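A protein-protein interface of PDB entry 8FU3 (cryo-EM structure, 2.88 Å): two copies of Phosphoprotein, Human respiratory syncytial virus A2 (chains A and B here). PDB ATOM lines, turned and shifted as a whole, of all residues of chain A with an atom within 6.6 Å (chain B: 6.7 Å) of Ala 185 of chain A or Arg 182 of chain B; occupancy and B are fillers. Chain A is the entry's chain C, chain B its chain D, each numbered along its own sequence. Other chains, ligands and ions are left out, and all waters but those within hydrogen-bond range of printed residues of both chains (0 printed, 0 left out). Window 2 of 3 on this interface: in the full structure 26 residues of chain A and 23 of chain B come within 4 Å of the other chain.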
ATOM      1  N   LYS A 180       1.206 -33.036   6.337  1.00  0.00           N
ATOM      2  CA  LYS A 180       1.299 -33.295   4.910  1.00  0.00           C
ATOM      3  C   LYS A 180       1.219 -31.985   4.137  1.00  0.00           C
ATOM      4  O   LYS A 180       1.974 -31.772   3.189  1.00  0.00           O
ATOM      5  CB  LYS A 180       0.207 -34.253   4.440  1.00  0.00           C
ATOM      6  CG  LYS A 180       0.298 -34.613   2.956  1.00  0.00           C
ATOM      7  CD  LYS A 180      -0.755 -35.638   2.553  1.00  0.00           C
ATOM      8  CE  LYS A 180      -0.738 -35.883   1.047  1.00  0.00           C
ATOM      9  NZ  LYS A 180       0.513 -36.563   0.605  1.00  0.00           N
ATOM     10  N   ILE A 181       0.314 -31.101   4.557  1.00  0.00           N
ATOM     11  CA  ILE A 181       0.177 -29.797   3.918  1.00  0.00           C
ATOM     12  C   ILE A 181       1.446 -28.975   4.078  1.00  0.00           C
ATOM     13  O   ILE A 181       1.915 -28.360   3.119  1.00  0.00           O
ATOM     14  CB  ILE A 181      -1.022 -29.011   4.485  1.00  0.00           C
ATOM     15  CG1 ILE A 181      -2.323 -29.693   4.070  1.00  0.00           C
ATOM     16  CG2 ILE A 181      -0.985 -27.573   3.988  1.00  0.00           C
ATOM     17  CD1 ILE A 181      -3.558 -29.197   4.810  1.00  0.00           C
ATOM     18  N   ARG A 182       2.005 -28.962   5.280  1.00  0.00           N
ATOM     19  CA  ARG A 182       3.236 -28.228   5.520  1.00  0.00           C
ATOM     20  C   ARG A 182       4.341 -28.802   4.664  1.00  0.00           C
ATOM     21  O   ARG A 182       5.139 -28.066   4.091  1.00  0.00           O
ATOM     22  CB  ARG A 182       3.652 -28.316   6.977  1.00  0.00           C
ATOM     23  CG  ARG A 182       2.741 -27.624   7.966  1.00  0.00           C
ATOM     24  CD  ARG A 182       3.146 -27.917   9.348  1.00  0.00           C
ATOM     25  NE  ARG A 182       4.361 -27.212   9.704  1.00  0.00           N
ATOM     26  CZ  ARG A 182       5.377 -27.730  10.425  1.00  0.00           C
ATOM     27  NH1 ARG A 182       5.328 -28.973  10.856  1.00  0.00           N
ATOM     28  NH2 ARG A 182       6.429 -26.991  10.696  1.00  0.00           N
ATOM     29  N   THR A 183       4.377 -30.125   4.563  1.00  0.00           N
ATOM     30  CA  THR A 183       5.396 -30.792   3.777  1.00  0.00           C
ATOM     31  C   THR A 183       5.315 -30.360   2.330  1.00  0.00           C
ATOM     32  O   THR A 183       6.329 -30.027   1.720  1.00  0.00           O
ATOM     33  CB  THR A 183       5.254 -32.322   3.875  1.00  0.00           C
ATOM     34  OG1 THR A 183       5.431 -32.733   5.238  1.00  0.00           O
ATOM     35  CG2 THR A 183       6.293 -33.001   3.004  1.00  0.00           C
ATOM     36  N   GLU A 184       4.106 -30.349   1.778  1.00  0.00           N
ATOM     37  CA  GLU A 184       3.917 -29.910   0.402  1.00  0.00           C
ATOM     38  C   GLU A 184       4.287 -28.448   0.239  1.00  0.00           C
ATOM     39  O   GLU A 184       4.967 -28.073  -0.712  1.00  0.00           O
ATOM     40  CB  GLU A 184       2.471 -30.121  -0.038  1.00  0.00           C
ATOM     41  CG  GLU A 184       2.196 -29.681  -1.472  1.00  0.00           C
ATOM     42  CD  GLU A 184       0.808 -30.001  -1.942  1.00  0.00           C
ATOM     43  OE1 GLU A 184       0.090 -30.663  -1.229  1.00  0.00           O
ATOM     44  OE2 GLU A 184       0.462 -29.579  -3.018  1.00  0.00           O
ATOM     45  N   ALA A 185       3.845 -27.618   1.176  1.00  0.00           N
ATOM     46  CA  ALA A 185       4.090 -26.183   1.115  1.00  0.00           C
ATOM     47  C   ALA A 185       5.570 -25.861   1.122  1.00  0.00           C
ATOM     48  O   ALA A 185       6.012 -24.904   0.494  1.00  0.00           O
ATOM     49  CB  ALA A 185       3.420 -25.496   2.289  1.00  0.00           C
ATOM     50  N   LEU A 186       6.340 -26.649   1.848  1.00  0.00           N
ATOM     51  CA  LEU A 186       7.761 -26.396   1.971  1.00  0.00           C
ATOM     52  C   LEU A 186       8.554 -27.132   0.905  1.00  0.00           C
ATOM     53  O   LEU A 186       9.784 -27.054   0.881  1.00  0.00           O
ATOM     54  CB  LEU A 186       8.225 -26.815   3.365  1.00  0.00           C
ATOM     55  CG  LEU A 186       7.549 -26.081   4.543  1.00  0.00           C
ATOM     56  CD1 LEU A 186       7.990 -26.730   5.838  1.00  0.00           C
ATOM     57  CD2 LEU A 186       7.915 -24.605   4.525  1.00  0.00           C
ATOM     58  N   MET A 187       7.849 -27.849   0.032  1.00  0.00           N
ATOM     59  CA  MET A 187       8.452 -28.619  -1.050  1.00  0.00           C
ATOM     60  C   MET A 187       7.555 -28.627  -2.278  1.00  0.00           C
ATOM     61  O   MET A 187       7.137 -29.689  -2.740  1.00  0.00           O
ATOM     62  CB  MET A 187       8.742 -30.050  -0.615  1.00  0.00           C
ATOM     63  CG  MET A 187       9.837 -30.197   0.420  1.00  0.00           C
ATOM     64  SD  MET A 187      11.420 -29.473  -0.127  1.00  0.00           S
ATOM     65  CE  MET A 187      11.856 -30.485  -1.545  1.00  0.00           C
ATOM     66  N   THR A 188       7.250 -27.444  -2.805  1.00  0.00           N
ATOM     67  CA  THR A 188       6.393 -27.354  -3.980  1.00  0.00           C
ATOM     68  C   THR A 188       7.229 -27.638  -5.216  1.00  0.00           C
ATOM     69  O   THR A 188       6.730 -28.148  -6.220  1.00  0.00           O
ATOM     70  CB  THR A 188       5.739 -25.967  -4.092  1.00  0.00           C
ATOM     71  OG1 THR A 188       6.763 -24.968  -4.225  1.00  0.00           O
ATOM     72  CG2 THR A 188       4.910 -25.683  -2.845  1.00  0.00           C
ATOM     73  N   ASN A 189       8.520 -27.344  -5.105  1.00  0.00           N
ATOM     74  CA  ASN A 189       9.504 -27.648  -6.131  1.00  0.00           C
ATOM     75  C   ASN A 189      10.694 -28.307  -5.451  1.00  0.00           C
ATOM     76  O   ASN A 189      10.590 -29.427  -4.952  1.00  0.00           O
ATOM     77  CB  ASN A 189       9.914 -26.392  -6.878  1.00  0.00           C
ATOM     78  CG  ASN A 189       8.828 -25.861  -7.773  1.00  0.00           C
ATOM     79  OD1 ASN A 189       8.508 -26.459  -8.808  1.00  0.00           O
ATOM     80  ND2 ASN A 189       8.253 -24.747  -7.396  1.00  0.00           N
ATOM     81  N   ARG A 191      11.878 -26.523  -3.000  1.00  0.00           N
ATOM     82  CA  ARG A 191      11.665 -25.764  -1.777  1.00  0.00           C
ATOM     83  C   ARG A 191      10.175 -25.588  -1.527  1.00  0.00           C
ATOM     84  O   ARG A 191       9.351 -25.822  -2.417  1.00  0.00           O
ATOM     85  CB  ARG A 191      12.304 -24.380  -1.873  1.00  0.00           C
ATOM     86  CG  ARG A 191      13.815 -24.332  -2.031  1.00  0.00           C
ATOM     87  CD  ARG A 191      14.537 -24.752  -0.795  1.00  0.00           C
ATOM     88  NE  ARG A 191      15.977 -24.580  -0.933  1.00  0.00           N
ATOM     89  CZ  ARG A 191      16.822 -25.463  -1.510  1.00  0.00           C
ATOM     90  NH1 ARG A 191      16.370 -26.593  -2.012  1.00  0.00           N
ATOM     91  NH2 ARG A 191      18.116 -25.184  -1.573  1.00  0.00           N
ATOM     92  N   MET B 177      -3.739 -22.415   3.218  1.00  0.00           N
ATOM     93  CA  MET B 177      -2.795 -22.809   4.250  1.00  0.00           C
ATOM     94  C   MET B 177      -1.412 -22.976   3.649  1.00  0.00           C
ATOM     95  O   MET B 177      -0.418 -22.574   4.253  1.00  0.00           O
ATOM     96  CB  MET B 177      -3.225 -24.097   4.943  1.00  0.00           C
ATOM     97  CG  MET B 177      -4.462 -23.968   5.829  1.00  0.00           C
ATOM     98  SD  MET B 177      -4.894 -25.511   6.642  1.00  0.00           S
ATOM     99  CE  MET B 177      -3.603 -25.624   7.890  1.00  0.00           C
ATOM    100  N   ILE B 178      -1.349 -23.526   2.440  1.00  0.00           N
ATOM    101  CA  ILE B 178      -0.071 -23.700   1.769  1.00  0.00           C
ATOM    102  C   ILE B 178       0.606 -22.366   1.511  1.00  0.00           C
ATOM    103  O   ILE B 178       1.794 -22.210   1.790  1.00  0.00           O
ATOM    104  CB  ILE B 178      -0.238 -24.463   0.435  1.00  0.00           C
ATOM    105  CG1 ILE B 178      -0.601 -25.924   0.727  1.00  0.00           C
ATOM    106  CG2 ILE B 178       1.024 -24.354  -0.419  1.00  0.00           C
ATOM    107  CD1 ILE B 178      -1.062 -26.715  -0.480  1.00  0.00           C
ATOM    108  N   GLU B 179      -0.143 -21.399   0.995  1.00  0.00           N
ATOM    109  CA  GLU B 179       0.436 -20.099   0.691  1.00  0.00           C
ATOM    110  C   GLU B 179       0.900 -19.376   1.948  1.00  0.00           C
ATOM    111  O   GLU B 179       1.957 -18.741   1.944  1.00  0.00           O
ATOM    112  CB  GLU B 179      -0.570 -19.242  -0.070  1.00  0.00           C
ATOM    113  CG  GLU B 179      -0.845 -19.737  -1.473  1.00  0.00           C
ATOM    114  CD  GLU B 179       0.377 -19.725  -2.338  1.00  0.00           C
ATOM    115  OE1 GLU B 179       0.939 -18.673  -2.523  1.00  0.00           O
ATOM    116  OE2 GLU B 179       0.763 -20.776  -2.795  1.00  0.00           O
ATOM    117  N   LYS B 180       0.135 -19.490   3.033  1.00  0.00           N
ATOM    118  CA  LYS B 180       0.527 -18.853   4.283  1.00  0.00           C
ATOM    119  C   LYS B 180       1.804 -19.483   4.823  1.00  0.00           C
ATOM    120  O   LYS B 180       2.712 -18.780   5.271  1.00  0.00           O
ATOM    121  CB  LYS B 180      -0.585 -18.954   5.324  1.00  0.00           C
ATOM    122  CG  LYS B 180      -0.282 -18.215   6.631  1.00  0.00           C
ATOM    123  CD  LYS B 180      -1.452 -18.285   7.588  1.00  0.00           C
ATOM    124  CE  LYS B 180      -1.238 -17.401   8.815  1.00  0.00           C
ATOM    125  NZ  LYS B 180      -0.073 -17.841   9.640  1.00  0.00           N
ATOM    126  N   ILE B 181       1.876 -20.809   4.756  1.00  0.00           N
ATOM    127  CA  ILE B 181       3.044 -21.544   5.215  1.00  0.00           C
ATOM    128  C   ILE B 181       4.259 -21.187   4.373  1.00  0.00           C
ATOM    129  O   ILE B 181       5.342 -20.948   4.910  1.00  0.00           O
ATOM    130  CB  ILE B 181       2.780 -23.061   5.166  1.00  0.00           C
ATOM    131  CG1 ILE B 181       1.716 -23.427   6.228  1.00  0.00           C
ATOM    132  CG2 ILE B 181       4.091 -23.838   5.399  1.00  0.00           C
ATOM    133  CD1 ILE B 181       1.095 -24.792   6.035  1.00  0.00           C
ATOM    134  N   ARG B 182       4.076 -21.138   3.054  1.00  0.00           N
ATOM    135  CA  ARG B 182       5.167 -20.765   2.168  1.00  0.00           C
ATOM    136  C   ARG B 182       5.665 -19.372   2.506  1.00  0.00           C
ATOM    137  O   ARG B 182       6.867 -19.128   2.538  1.00  0.00           O
ATOM    138  CB  ARG B 182       4.729 -20.776   0.711  1.00  0.00           C
ATOM    139  CG  ARG B 182       4.493 -22.137   0.109  1.00  0.00           C
ATOM    140  CD  ARG B 182       3.950 -22.038  -1.260  1.00  0.00           C
ATOM    141  NE  ARG B 182       4.965 -21.610  -2.206  1.00  0.00           N
ATOM    142  CZ  ARG B 182       4.721 -21.072  -3.420  1.00  0.00           C
ATOM    143  NH1 ARG B 182       3.487 -20.886  -3.843  1.00  0.00           N
ATOM    144  NH2 ARG B 182       5.736 -20.733  -4.199  1.00  0.00           N
ATOM    145  N   THR B 183       4.734 -18.465   2.776  1.00  0.00           N
ATOM    146  CA  THR B 183       5.083 -17.092   3.091  1.00  0.00           C
ATOM    147  C   THR B 183       5.936 -17.011   4.347  1.00  0.00           C
ATOM    148  O   THR B 183       6.976 -16.352   4.358  1.00  0.00           O
ATOM    149  CB  THR B 183       3.812 -16.241   3.272  1.00  0.00           C
ATOM    150  OG1 THR B 183       3.069 -16.226   2.044  1.00  0.00           O
ATOM    151  CG2 THR B 183       4.175 -14.820   3.659  1.00  0.00           C
ATOM    152  N   GLU B 184       5.519 -17.704   5.399  1.00  0.00           N
ATOM    153  CA  GLU B 184       6.256 -17.691   6.657  1.00  0.00           C
ATOM    154  C   GLU B 184       7.645 -18.288   6.473  1.00  0.00           C
ATOM    155  O   GLU B 184       8.621 -17.841   7.077  1.00  0.00           O
ATOM    156  CB  GLU B 184       5.483 -18.458   7.725  1.00  0.00           C
ATOM    157  CG  GLU B 184       4.207 -17.771   8.168  1.00  0.00           C
ATOM    158  CD  GLU B 184       3.371 -18.625   9.059  1.00  0.00           C
ATOM    159  OE1 GLU B 184       3.692 -19.776   9.220  1.00  0.00           O
ATOM    160  OE2 GLU B 184       2.401 -18.126   9.583  1.00  0.00           O
ATOM    161  N   ALA B 185       7.737 -19.285   5.605  1.00  0.00           N
ATOM    162  CA  ALA B 185       8.994 -19.960   5.323  1.00  0.00           C
ATOM    163  C   ALA B 185       9.991 -19.040   4.620  1.00  0.00           C
ATOM    164  O   ALA B 185      11.168 -19.380   4.499  1.00  0.00           O
ATOM    165  CB  ALA B 185       8.740 -21.188   4.470  1.00  0.00           C
ATOM    166  N   LEU B 186       9.517 -17.904   4.114  1.00  0.00           N
ATOM    167  CA  LEU B 186      10.364 -16.984   3.374  1.00  0.00           C
ATOM    168  C   LEU B 186      10.711 -15.733   4.172  1.00  0.00           C
ATOM    169  O   LEU B 186      11.228 -14.766   3.614  1.00  0.00           O
ATOM    170  CB  LEU B 186       9.681 -16.590   2.058  1.00  0.00           C
ATOM    171  CG  LEU B 186       9.431 -17.739   1.061  1.00  0.00           C
ATOM    172  CD1 LEU B 186       8.585 -17.223  -0.095  1.00  0.00           C
ATOM    173  CD2 LEU B 186      10.762 -18.281   0.549  1.00  0.00           C
ATOM    174  N   MET B 187      10.457 -15.750   5.481  1.00  0.00           N
ATOM    175  CA  MET B 187      10.800 -14.592   6.306  1.00  0.00           C
ATOM    176  C   MET B 187      12.301 -14.324   6.295  1.00  0.00           C
ATOM    177  O   MET B 187      12.732 -13.173   6.378  1.00  0.00           O
ATOM    178  CB  MET B 187      10.326 -14.774   7.749  1.00  0.00           C
ATOM    179  CG  MET B 187       8.815 -14.762   7.949  1.00  0.00           C
ATOM    180  SD  MET B 187       8.040 -13.221   7.435  1.00  0.00           S
ATOM    181  CE  MET B 187       7.354 -13.692   5.849  1.00  0.00           C
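Arg 182 of chain A touches Ile 181 of chain B, but with the chains exchanged Ile 181 of chain A does not touch Arg 182 of chain B (7.4 Å). Ala 185 of chain A touches Ile 181 of chain B, but with the chains exchanged Ile 181 of chain A does not touch Ala 185 of chain B (10.0 Å). Ala 185 of chain A touches Arg 182 of chain B, but with the chains exchanged Arg 182 of chain A does not touch Ala 185 of chain B (7.8 Å). Leu 186 of chain A touches Ile 181 of chain B, but with the chains exchanged Ile 181 of chain A does not touch Leu 186 of chain B (13.0 Å). Positions printed for both chains: 180, 181, 182, 183, 184, 185, 186 and 187. Of the 7 pairs that touch across the chains among the printed residues, none has its exchanged pair printed and touching as well.
OE2 of Glu 179 of chain B lies within salt-bridge range of NH1 of Arg 182 of chain B.
Of the 11 printed residues of chain A, 4 touch a printed residue of chain B. Hydrophobic or aromatic side chains of chain A that line the printed part of chain B: Ile 181, Ala 185 and Leu 186. Hydrophobic or aromatic side chains of chain B within 4 Å of the printed part of chain A: Ile 178, Ile 181 and Ala 185. Among the printed residues, 7 pairs touch across the chains.
Of chain B, only Ile 178 (3.7 Å), Ile 181 (3.6 Å) and Arg 182 (3.2 Å) come within 4 Å of Ala 185 of chain A. Arg 182 of chain B touches one residue of chain A. Of the printed residues of chain A, Ala 185 of chain B touches Leu 186 (3.5 Å). Printed residues of chain B within 4 Å of Leu 186 of chain A: Ile 181 (3.997 Å) and Ala 185 (3.5 Å). Thr 188 of chain A touches none of the printed residues of chain B.
Among the printed residues, pairs that only touch across the chains: Ile 181 of chain A with Ile 178 of chain B (3.7 Å), Arg 182 of chain A with Ile 181 of chain B (3.8 Å), Ala 185 of chain A with Ile 178 of chain B (3.7 Å), Ala 185 of chain A with Ile 181 of chain B (3.6 Å), Ala 185 of chain A with Arg 182 of chain B (3.2 Å), Leu 186 of chain A with Ile 181 of chain B (3.997 Å) and Leu 186 of chain A with Ala 185 of chain B (3.5 Å).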
